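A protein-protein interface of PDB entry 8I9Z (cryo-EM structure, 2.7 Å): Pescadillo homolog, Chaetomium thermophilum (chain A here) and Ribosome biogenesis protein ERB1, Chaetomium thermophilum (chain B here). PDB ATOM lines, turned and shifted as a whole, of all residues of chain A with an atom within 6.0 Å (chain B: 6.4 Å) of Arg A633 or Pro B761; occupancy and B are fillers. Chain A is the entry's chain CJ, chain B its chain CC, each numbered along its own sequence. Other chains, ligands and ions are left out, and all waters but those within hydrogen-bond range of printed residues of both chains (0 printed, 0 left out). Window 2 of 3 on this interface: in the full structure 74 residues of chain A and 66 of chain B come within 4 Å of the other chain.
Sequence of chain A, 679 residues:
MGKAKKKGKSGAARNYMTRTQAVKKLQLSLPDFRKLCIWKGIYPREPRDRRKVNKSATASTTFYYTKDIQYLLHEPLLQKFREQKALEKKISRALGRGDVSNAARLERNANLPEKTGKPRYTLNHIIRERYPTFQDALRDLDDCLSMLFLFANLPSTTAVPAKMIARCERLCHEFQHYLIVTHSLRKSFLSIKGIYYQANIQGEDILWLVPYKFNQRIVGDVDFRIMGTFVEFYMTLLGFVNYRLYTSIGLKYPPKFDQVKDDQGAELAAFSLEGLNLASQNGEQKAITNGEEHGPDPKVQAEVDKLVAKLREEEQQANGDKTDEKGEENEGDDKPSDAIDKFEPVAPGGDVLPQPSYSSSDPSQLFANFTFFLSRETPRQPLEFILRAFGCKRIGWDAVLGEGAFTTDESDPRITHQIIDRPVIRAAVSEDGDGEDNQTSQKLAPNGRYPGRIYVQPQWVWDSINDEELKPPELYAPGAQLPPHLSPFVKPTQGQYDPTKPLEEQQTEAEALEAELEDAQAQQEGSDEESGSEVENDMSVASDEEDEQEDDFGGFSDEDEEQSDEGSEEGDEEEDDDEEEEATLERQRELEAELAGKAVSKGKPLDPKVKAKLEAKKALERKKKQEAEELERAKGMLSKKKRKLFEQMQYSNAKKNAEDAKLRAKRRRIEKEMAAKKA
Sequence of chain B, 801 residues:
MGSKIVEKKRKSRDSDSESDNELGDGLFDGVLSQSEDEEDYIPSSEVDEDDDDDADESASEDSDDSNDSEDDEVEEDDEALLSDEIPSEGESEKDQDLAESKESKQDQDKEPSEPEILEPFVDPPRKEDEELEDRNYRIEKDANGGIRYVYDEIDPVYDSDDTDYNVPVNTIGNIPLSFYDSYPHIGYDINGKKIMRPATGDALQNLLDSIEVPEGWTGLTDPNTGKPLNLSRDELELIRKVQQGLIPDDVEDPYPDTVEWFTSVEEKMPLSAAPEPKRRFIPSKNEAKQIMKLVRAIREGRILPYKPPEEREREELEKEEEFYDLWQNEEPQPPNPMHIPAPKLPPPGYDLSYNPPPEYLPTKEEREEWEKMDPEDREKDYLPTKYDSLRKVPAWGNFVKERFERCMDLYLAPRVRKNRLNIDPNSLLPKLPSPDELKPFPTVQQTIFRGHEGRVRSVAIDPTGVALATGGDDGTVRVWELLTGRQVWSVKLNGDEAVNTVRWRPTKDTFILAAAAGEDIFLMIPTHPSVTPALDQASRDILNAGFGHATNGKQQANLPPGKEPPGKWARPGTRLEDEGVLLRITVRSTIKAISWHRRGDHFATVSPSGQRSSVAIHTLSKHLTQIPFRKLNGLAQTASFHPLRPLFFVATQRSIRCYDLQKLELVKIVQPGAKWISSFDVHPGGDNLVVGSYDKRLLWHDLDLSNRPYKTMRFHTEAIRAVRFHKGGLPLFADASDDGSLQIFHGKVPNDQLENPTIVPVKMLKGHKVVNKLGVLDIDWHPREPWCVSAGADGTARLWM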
ATOM      1  N   ALA A 628     -28.540 -26.351  13.045  1.00  0.00           N
ATOM      2  CA  ALA A 628     -28.339 -26.569  14.474  1.00  0.00           C
ATOM      3  C   ALA A 628     -26.893 -26.322  14.875  1.00  0.00           C
ATOM      4  O   ALA A 628     -26.622 -25.821  15.972  1.00  0.00           O
ATOM      5  CB  ALA A 628     -28.768 -27.986  14.855  1.00  0.00           C
ATOM      6  N   GLU A 629     -25.949 -26.682  14.005  1.00  0.00           N
ATOM      7  CA  GLU A 629     -24.544 -26.391  14.268  1.00  0.00           C
ATOM      8  C   GLU A 629     -24.275 -24.892  14.232  1.00  0.00           C
ATOM      9  O   GLU A 629     -23.507 -24.368  15.045  1.00  0.00           O
ATOM     10  CB  GLU A 629     -23.660 -27.121  13.258  1.00  0.00           C
ATOM     11  CG  GLU A 629     -23.068 -28.422  13.772  1.00  0.00           C
ATOM     12  CD  GLU A 629     -21.732 -28.743  13.133  1.00  0.00           C
ATOM     13  OE1 GLU A 629     -21.162 -27.856  12.464  1.00  0.00           O
ATOM     14  OE2 GLU A 629     -21.250 -29.884  13.301  1.00  0.00           O
ATOM     15  N   GLU A 630     -24.896 -24.186  13.284  1.00  0.00           N
ATOM     16  CA  GLU A 630     -24.706 -22.742  13.196  1.00  0.00           C
ATOM     17  C   GLU A 630     -25.347 -22.025  14.374  1.00  0.00           C
ATOM     18  O   GLU A 630     -24.835 -21.001  14.839  1.00  0.00           O
ATOM     19  CB  GLU A 630     -25.273 -22.215  11.881  1.00  0.00           C
ATOM     20  CG  GLU A 630     -24.229 -21.956  10.811  1.00  0.00           C
ATOM     21  CD  GLU A 630     -24.573 -20.762   9.941  1.00  0.00           C
ATOM     22  OE1 GLU A 630     -25.668 -20.189  10.124  1.00  0.00           O
ATOM     23  OE2 GLU A 630     -23.749 -20.396   9.077  1.00  0.00           O
ATOM     24  N   LEU A 631     -26.479 -22.538  14.857  1.00  0.00           N
ATOM     25  CA  LEU A 631     -27.122 -21.950  16.027  1.00  0.00           C
ATOM     26  C   LEU A 631     -26.277 -22.148  17.276  1.00  0.00           C
ATOM     27  O   LEU A 631     -26.184 -21.250  18.119  1.00  0.00           O
ATOM     28  CB  LEU A 631     -28.513 -22.554  16.210  1.00  0.00           C
ATOM     29  CG  LEU A 631     -29.507 -21.841  17.126  1.00  0.00           C
ATOM     30  CD1 LEU A 631     -30.895 -21.882  16.522  1.00  0.00           C
ATOM     31  CD2 LEU A 631     -29.522 -22.475  18.501  1.00  0.00           C
ATOM     32  N   GLU A 632     -25.653 -23.319  17.413  1.00  0.00           N
ATOM     33  CA  GLU A 632     -24.878 -23.618  18.613  1.00  0.00           C
ATOM     34  C   GLU A 632     -23.597 -22.800  18.670  1.00  0.00           C
ATOM     35  O   GLU A 632     -23.122 -22.458  19.759  1.00  0.00           O
ATOM     36  CB  GLU A 632     -24.561 -25.110  18.673  1.00  0.00           C
ATOM     37  CG  GLU A 632     -25.498 -25.911  19.556  1.00  0.00           C
ATOM     38  CD  GLU A 632     -24.879 -27.211  20.031  1.00  0.00           C
ATOM     39  OE1 GLU A 632     -23.814 -27.592  19.500  1.00  0.00           O
ATOM     40  OE2 GLU A 632     -25.457 -27.853  20.933  1.00  0.00           O
ATOM     41  N   ARG A 633     -23.010 -22.492  17.513  1.00  0.00           N
ATOM     42  CA  ARG A 633     -21.790 -21.693  17.494  1.00  0.00           C
ATOM     43  C   ARG A 633     -22.065 -20.254  17.915  1.00  0.00           C
ATOM     44  O   ARG A 633     -21.304 -19.665  18.689  1.00  0.00           O
ATOM     45  CB  ARG A 633     -21.158 -21.730  16.106  1.00  0.00           C
ATOM     46  CG  ARG A 633     -20.572 -23.070  15.716  1.00  0.00           C
ATOM     47  CD  ARG A 633     -19.570 -22.897  14.596  1.00  0.00           C
ATOM     48  NE  ARG A 633     -20.132 -22.125  13.498  1.00  0.00           N
ATOM     49  CZ  ARG A 633     -19.455 -21.240  12.783  1.00  0.00           C
ATOM     50  NH1 ARG A 633     -18.180 -20.987  13.024  1.00  0.00           N
ATOM     51  NH2 ARG A 633     -20.074 -20.584  11.806  1.00  0.00           N
ATOM     52  N   ALA A 634     -23.151 -19.669  17.407  1.00  0.00           N
ATOM     53  CA  ALA A 634     -23.467 -18.285  17.740  1.00  0.00           C
ATOM     54  C   ALA A 634     -24.042 -18.169  19.144  1.00  0.00           C
ATOM     55  O   ALA A 634     -23.970 -17.100  19.763  1.00  0.00           O
ATOM     56  CB  ALA A 634     -24.438 -17.706  16.713  1.00  0.00           C
ATOM     57  N   LYS A 635     -24.630 -19.250  19.658  1.00  0.00           N
ATOM     58  CA  LYS A 635     -25.140 -19.234  21.025  1.00  0.00           C
ATOM     59  C   LYS A 635     -24.002 -19.196  22.032  1.00  0.00           C
ATOM     60  O   LYS A 635     -24.156 -18.667  23.138  1.00  0.00           O
ATOM     61  CB  LYS A 635     -26.032 -20.450  21.270  1.00  0.00           C
ATOM     62  CG  LYS A 635     -27.026 -20.282  22.396  1.00  0.00           C
ATOM     63  CD  LYS A 635     -28.200 -21.220  22.234  1.00  0.00           C
ATOM     64  CE  LYS A 635     -27.830 -22.643  22.582  1.00  0.00           C
ATOM     65  NZ  LYS A 635     -27.446 -22.777  24.009  1.00  0.00           N
ATOM     66  N   GLY A 636     -22.849 -19.756  21.667  1.00  0.00           N
ATOM     67  CA  GLY A 636     -21.723 -19.769  22.584  1.00  0.00           C
ATOM     68  C   GLY A 636     -21.046 -18.420  22.711  1.00  0.00           C
ATOM     69  O   GLY A 636     -20.392 -18.134  23.716  1.00  0.00           O
ATOM     70  N   MET A 637     -21.189 -17.574  21.692  1.00  0.00           N
ATOM     71  CA  MET A 637     -20.592 -16.245  21.740  1.00  0.00           C
ATOM     72  C   MET A 637     -21.331 -15.324  22.700  1.00  0.00           C
ATOM     73  O   MET A 637     -20.776 -14.306  23.129  1.00  0.00           O
ATOM     74  CB  MET A 637     -20.569 -15.637  20.336  1.00  0.00           C
ATOM     75  CG  MET A 637     -19.372 -15.929  19.386  1.00  0.00           C
ATOM     76  SD  MET A 637     -17.648 -16.023  19.940  1.00  0.00           S
ATOM     77  CE  MET A 637     -17.503 -17.642  20.685  1.00  0.00           C
ATOM     78  N   PRO B 430     -24.943 -13.147  17.260  1.00  0.00           N
ATOM     79  CA  PRO B 430     -23.942 -12.515  16.399  1.00  0.00           C
ATOM     80  C   PRO B 430     -23.757 -13.288  15.101  1.00  0.00           C
ATOM     81  O   PRO B 430     -24.198 -14.426  14.947  1.00  0.00           O
ATOM     82  CB  PRO B 430     -22.674 -12.552  17.251  1.00  0.00           C
ATOM     83  CG  PRO B 430     -22.846 -13.736  18.105  1.00  0.00           C
ATOM     84  CD  PRO B 430     -24.319 -13.870  18.381  1.00  0.00           C
ATOM     85  N   LEU B 432     -21.131 -14.955  12.505  1.00  0.00           N
ATOM     86  CA  LEU B 432     -19.831 -15.595  12.505  1.00  0.00           C
ATOM     87  C   LEU B 432     -19.502 -16.070  11.100  1.00  0.00           C
ATOM     88  O   LEU B 432     -20.390 -16.530  10.376  1.00  0.00           O
ATOM     89  CB  LEU B 432     -19.815 -16.789  13.467  1.00  0.00           C
ATOM     90  CG  LEU B 432     -19.706 -16.473  14.955  1.00  0.00           C
ATOM     91  CD1 LEU B 432     -19.747 -17.753  15.768  1.00  0.00           C
ATOM     92  CD2 LEU B 432     -18.439 -15.690  15.243  1.00  0.00           C
ATOM     93  N   PRO B 433     -18.244 -15.966  10.683  1.00  0.00           N
ATOM     94  CA  PRO B 433     -17.859 -16.461   9.360  1.00  0.00           C
ATOM     95  C   PRO B 433     -17.869 -17.983   9.318  1.00  0.00           C
ATOM     96  O   PRO B 433     -17.749 -18.664  10.335  1.00  0.00           O
ATOM     97  CB  PRO B 433     -16.446 -15.909   9.154  1.00  0.00           C
ATOM     98  CG  PRO B 433     -15.966 -15.494  10.483  1.00  0.00           C
ATOM     99  CD  PRO B 433     -17.094 -15.477  11.458  1.00  0.00           C
ATOM    100  N   SER B 434     -18.036 -18.501   8.108  1.00  0.00           N
ATOM    101  CA  SER B 434     -18.115 -19.942   7.898  1.00  0.00           C
ATOM    102  C   SER B 434     -16.772 -20.588   8.212  1.00  0.00           C
ATOM    103  O   SER B 434     -15.727 -20.010   7.901  1.00  0.00           O
ATOM    104  CB  SER B 434     -18.519 -20.252   6.463  1.00  0.00           C
ATOM    105  OG  SER B 434     -17.910 -21.450   6.012  1.00  0.00           O
ATOM    106  N   PRO B 435     -16.759 -21.762   8.844  1.00  0.00           N
ATOM    107  CA  PRO B 435     -15.477 -22.416   9.145  1.00  0.00           C
ATOM    108  C   PRO B 435     -14.734 -22.900   7.914  1.00  0.00           C
ATOM    109  O   PRO B 435     -13.528 -23.162   7.999  1.00  0.00           O
ATOM    110  CB  PRO B 435     -15.884 -23.581  10.056  1.00  0.00           C
ATOM    111  CG  PRO B 435     -17.312 -23.816   9.763  1.00  0.00           C
ATOM    112  CD  PRO B 435     -17.900 -22.487   9.420  1.00  0.00           C
ATOM    113  N   LEU B 438     -12.141 -20.554   7.106  1.00  0.00           N
ATOM    114  CA  LEU B 438     -11.162 -20.419   8.173  1.00  0.00           C
ATOM    115  C   LEU B 438     -10.241 -21.628   8.284  1.00  0.00           C
ATOM    116  O   LEU B 438      -9.621 -21.826   9.331  1.00  0.00           O
ATOM    117  CB  LEU B 438     -11.884 -20.174   9.497  1.00  0.00           C
ATOM    118  CG  LEU B 438     -12.263 -18.720   9.789  1.00  0.00           C
ATOM    119  CD1 LEU B 438     -12.655 -18.542  11.241  1.00  0.00           C
ATOM    120  CD2 LEU B 438     -11.135 -17.770   9.425  1.00  0.00           C
ATOM    121  N   MET B 713     -17.298 -16.777  26.845  1.00  0.00           N
ATOM    122  CA  MET B 713     -17.748 -17.848  25.968  1.00  0.00           C
ATOM    123  C   MET B 713     -18.091 -19.096  26.770  1.00  0.00           C
ATOM    124  O   MET B 713     -17.459 -19.394  27.786  1.00  0.00           O
ATOM    125  CB  MET B 713     -16.657 -18.169  24.936  1.00  0.00           C
ATOM    126  CG  MET B 713     -16.242 -16.983  24.075  1.00  0.00           C
ATOM    127  SD  MET B 713     -14.469 -16.842  23.815  1.00  0.00           S
ATOM    128  CE  MET B 713     -14.124 -18.352  22.947  1.00  0.00           C
ATOM    129  N   PHE B 715     -19.174 -23.258  25.702  1.00  0.00           N
ATOM    130  CA  PHE B 715     -19.487 -24.258  24.696  1.00  0.00           C
ATOM    131  C   PHE B 715     -19.613 -25.664  25.255  1.00  0.00           C
ATOM    132  O   PHE B 715     -19.851 -26.593  24.478  1.00  0.00           O
ATOM    133  CB  PHE B 715     -18.428 -24.253  23.591  1.00  0.00           C
ATOM    134  CG  PHE B 715     -18.573 -23.126  22.628  1.00  0.00           C
ATOM    135  CD1 PHE B 715     -19.469 -23.203  21.581  1.00  0.00           C
ATOM    136  CD2 PHE B 715     -17.801 -21.989  22.761  1.00  0.00           C
ATOM    137  CE1 PHE B 715     -19.601 -22.161  20.693  1.00  0.00           C
ATOM    138  CE2 PHE B 715     -17.929 -20.953  21.877  1.00  0.00           C
ATOM    139  CZ  PHE B 715     -18.829 -21.038  20.841  1.00  0.00           C
ATOM    140  N   GLN B 743     -12.887 -28.390  21.717  1.00  0.00           N
ATOM    141  CA  GLN B 743     -13.399 -27.359  20.830  1.00  0.00           C
ATOM    142  C   GLN B 743     -12.253 -26.496  20.321  1.00  0.00           C
ATOM    143  O   GLN B 743     -11.440 -26.005  21.109  1.00  0.00           O
ATOM    144  CB  GLN B 743     -14.438 -26.506  21.552  1.00  0.00           C
ATOM    145  CG  GLN B 743     -14.765 -25.220  20.851  1.00  0.00           C
ATOM    146  CD  GLN B 743     -15.859 -25.374  19.822  1.00  0.00           C
ATOM    147  OE1 GLN B 743     -16.992 -25.715  20.154  1.00  0.00           O
ATOM    148  NE2 GLN B 743     -15.528 -25.122  18.563  1.00  0.00           N
ATOM    149  N   ILE B 744     -12.199 -26.312  19.006  1.00  0.00           N
ATOM    150  CA  ILE B 744     -11.130 -25.576  18.344  1.00  0.00           C
ATOM    151  C   ILE B 744     -11.656 -24.194  17.992  1.00  0.00           C
ATOM    152  O   ILE B 744     -12.814 -24.050  17.585  1.00  0.00           O
ATOM    153  CB  ILE B 744     -10.632 -26.310  17.087  1.00  0.00           C
ATOM    154  CG1 ILE B 744     -10.458 -27.801  17.367  1.00  0.00           C
ATOM    155  CG2 ILE B 744      -9.323 -25.719  16.602  1.00  0.00           C
ATOM    156  CD1 ILE B 744      -9.377 -28.109  18.357  1.00  0.00           C
ATOM    157  N   PHE B 745     -10.816 -23.178  18.164  1.00  0.00           N
ATOM    158  CA  PHE B 745     -11.164 -21.813  17.806  1.00  0.00           C
ATOM    159  C   PHE B 745     -10.140 -21.252  16.835  1.00  0.00           C
ATOM    160  O   PHE B 745      -8.995 -21.710  16.791  1.00  0.00           O
ATOM    161  CB  PHE B 745     -11.224 -20.891  19.018  1.00  0.00           C
ATOM    162  CG  PHE B 745     -12.240 -21.277  20.036  1.00  0.00           C
ATOM    163  CD1 PHE B 745     -11.922 -22.147  21.060  1.00  0.00           C
ATOM    164  CD2 PHE B 745     -13.523 -20.781  19.965  1.00  0.00           C
ATOM    165  CE1 PHE B 745     -12.860 -22.497  21.996  1.00  0.00           C
ATOM    166  CE2 PHE B 745     -14.467 -21.146  20.888  1.00  0.00           C
ATOM    167  CZ  PHE B 745     -14.131 -21.987  21.914  1.00  0.00           C
ATOM    168  N   HIS B 746     -10.556 -20.253  16.066  1.00  0.00           N
ATOM    169  CA  HIS B 746      -9.645 -19.487  15.229  1.00  0.00           C
ATOM    170  C   HIS B 746      -9.455 -18.123  15.876  1.00  0.00           C
ATOM    171  O   HIS B 746     -10.334 -17.260  15.792  1.00  0.00           O
ATOM    172  CB  HIS B 746     -10.190 -19.360  13.810  1.00  0.00           C
ATOM    173  CG  HIS B 746      -9.508 -18.316  12.984  1.00  0.00           C
ATOM    174  ND1 HIS B 746      -9.914 -17.000  12.954  1.00  0.00           N
ATOM    175  CD2 HIS B 746      -8.454 -18.401  12.139  1.00  0.00           C
ATOM    176  CE1 HIS B 746      -9.134 -16.318  12.137  1.00  0.00           C
ATOM    177  NE2 HIS B 746      -8.240 -17.145  11.629  1.00  0.00           N
ATOM    178  N   ILE B 759     -12.260 -13.877  17.365  1.00  0.00           N
ATOM    179  CA  ILE B 759     -12.363 -15.197  17.974  1.00  0.00           C
ATOM    180  C   ILE B 759     -13.596 -15.882  17.408  1.00  0.00           C
ATOM    181  O   ILE B 759     -14.720 -15.413  17.613  1.00  0.00           O
ATOM    182  CB  ILE B 759     -12.433 -15.121  19.504  1.00  0.00           C
ATOM    183  CG1 ILE B 759     -11.134 -14.558  20.076  1.00  0.00           C
ATOM    184  CG2 ILE B 759     -12.698 -16.489  20.081  1.00  0.00           C
ATOM    185  CD1 ILE B 759     -11.213 -13.104  20.473  1.00  0.00           C
ATOM    186  N   VAL B 760     -13.384 -16.982  16.689  1.00  0.00           N
ATOM    187  CA  VAL B 760     -14.461 -17.720  16.030  1.00  0.00           C
ATOM    188  C   VAL B 760     -14.284 -19.212  16.289  1.00  0.00           C
ATOM    189  O   VAL B 760     -13.194 -19.749  16.047  1.00  0.00           O
ATOM    190  CB  VAL B 760     -14.487 -17.436  14.519  1.00  0.00           C
ATOM    191  CG1 VAL B 760     -15.481 -18.342  13.820  1.00  0.00           C
ATOM    192  CG2 VAL B 760     -14.816 -15.983  14.242  1.00  0.00           C
ATOM    193  N   PRO B 761     -15.304 -19.919  16.780  1.00  0.00           N
ATOM    194  CA  PRO B 761     -15.204 -21.382  16.886  1.00  0.00           C
ATOM    195  C   PRO B 761     -15.250 -22.031  15.511  1.00  0.00           C
ATOM    196  O   PRO B 761     -15.988 -21.592  14.628  1.00  0.00           O
ATOM    197  CB  PRO B 761     -16.421 -21.758  17.732  1.00  0.00           C
ATOM    198  CG  PRO B 761     -17.392 -20.672  17.481  1.00  0.00           C
ATOM    199  CD  PRO B 761     -16.601 -19.420  17.261  1.00  0.00           C
ATOM    200  N   VAL B 762     -14.449 -23.078  15.328  1.00  0.00           N
ATOM    201  CA  VAL B 762     -14.335 -23.680  14.005  1.00  0.00           C
ATOM    202  C   VAL B 762     -14.712 -25.157  13.997  1.00  0.00           C
ATOM    203  O   VAL B 762     -15.206 -25.663  12.984  1.00  0.00           O
ATOM    204  CB  VAL B 762     -12.920 -23.479  13.433  1.00  0.00           C
ATOM    205  CG1 VAL B 762     -12.719 -22.034  13.027  1.00  0.00           C
ATOM    206  CG2 VAL B 762     -11.871 -23.899  14.435  1.00  0.00           C
ATOM    207  N   LYS B 763     -14.513 -25.858  15.111  1.00  0.00           N
ATOM    208  CA  LYS B 763     -14.721 -27.301  15.094  1.00  0.00           C
ATOM    209  C   LYS B 763     -14.923 -27.829  16.507  1.00  0.00           C
ATOM    210  O   LYS B 763     -14.305 -27.338  17.454  1.00  0.00           O
ATOM    211  CB  LYS B 763     -13.533 -28.014  14.432  1.00  0.00           C
ATOM    212  CG  LYS B 763     -13.763 -29.481  14.115  1.00  0.00           C
ATOM    213  CD  LYS B 763     -15.024 -29.664  13.294  1.00  0.00           C
ATOM    214  CE  LYS B 763     -15.184 -31.101  12.840  1.00  0.00           C
ATOM    215  NZ  LYS B 763     -16.201 -31.825  13.652  1.00  0.00           N
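Glu A632 touches Phe B715 (O to CE1, 3.7 Å). Leu B432 touches Arg A633. Arg A633 touches Pro B435. CG1 of Val B760 touches NH1 of Arg A633 (3.9 Å). Ala A634 touches Pro B430 (O to CD, 3.5 Å). Gly A636 touches Met B713. Phe B715 touches Gly A636. Pro B430 touches Met A637. CG of Met B713 touches CE of Met A637 (3.7 Å). Pro B761 touches Met A637 (CD to CE, 3.96 Å).
Of the 10 printed residues of chain A, 5 touch a printed residue of chain B. Hydrophobic or aromatic side chains of chain A that line the printed part of chain B: Ala A634 and Met A637. Of the 17 printed residues of chain B, 9 touch a printed residue of chain A. Hydrophobic or aromatic side chains of chain B that line the printed part of chain A: Pro B430, Leu B432, Pro B435, Met B713, Phe B715, Val B760 and Pro B761. Among the printed residues, 15 pairs touch across the chains.
Arg A633 touches six residues of chain B. Of chain A, only Arg A633 (2.8 Å) and Met A637 (3.96 Å) come within 4 Å of Pro B761. Of the printed residues of chain A, Pro B433 touches Arg A633. Of the printed residues of chain A, Val B760 touches Arg A633 (3.9 Å). Of the printed residues of chain A, Leu B432 touches Arg A633 (3.8 Å). The nearest residue of chain A that does not touch Pro B761 is Ala A634 (5.8 Å). The nearest printed residue of chain A that does not touch Pro B435 is Glu A629 (6.2 Å).
The guanidinium group (NH2) of Arg A633 lies within hydrogen-bond range of the backbone carbonyl oxygen (O) of Pro B433, at 3.4 Å. NH1 of Arg A633 is in hydrogen-bond range of O of Pro B761 (2.8 Å). The backbone carbonyl oxygen (O) of Ile B759 lies close to the side-chain sulfur (SD) of Met A637, 3.8 Å away.
The backbone NH (N) of His B746 lies within hydrogen-bond range of the backbone carbonyl oxygen (O) of Val B760 (2.7 Å).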
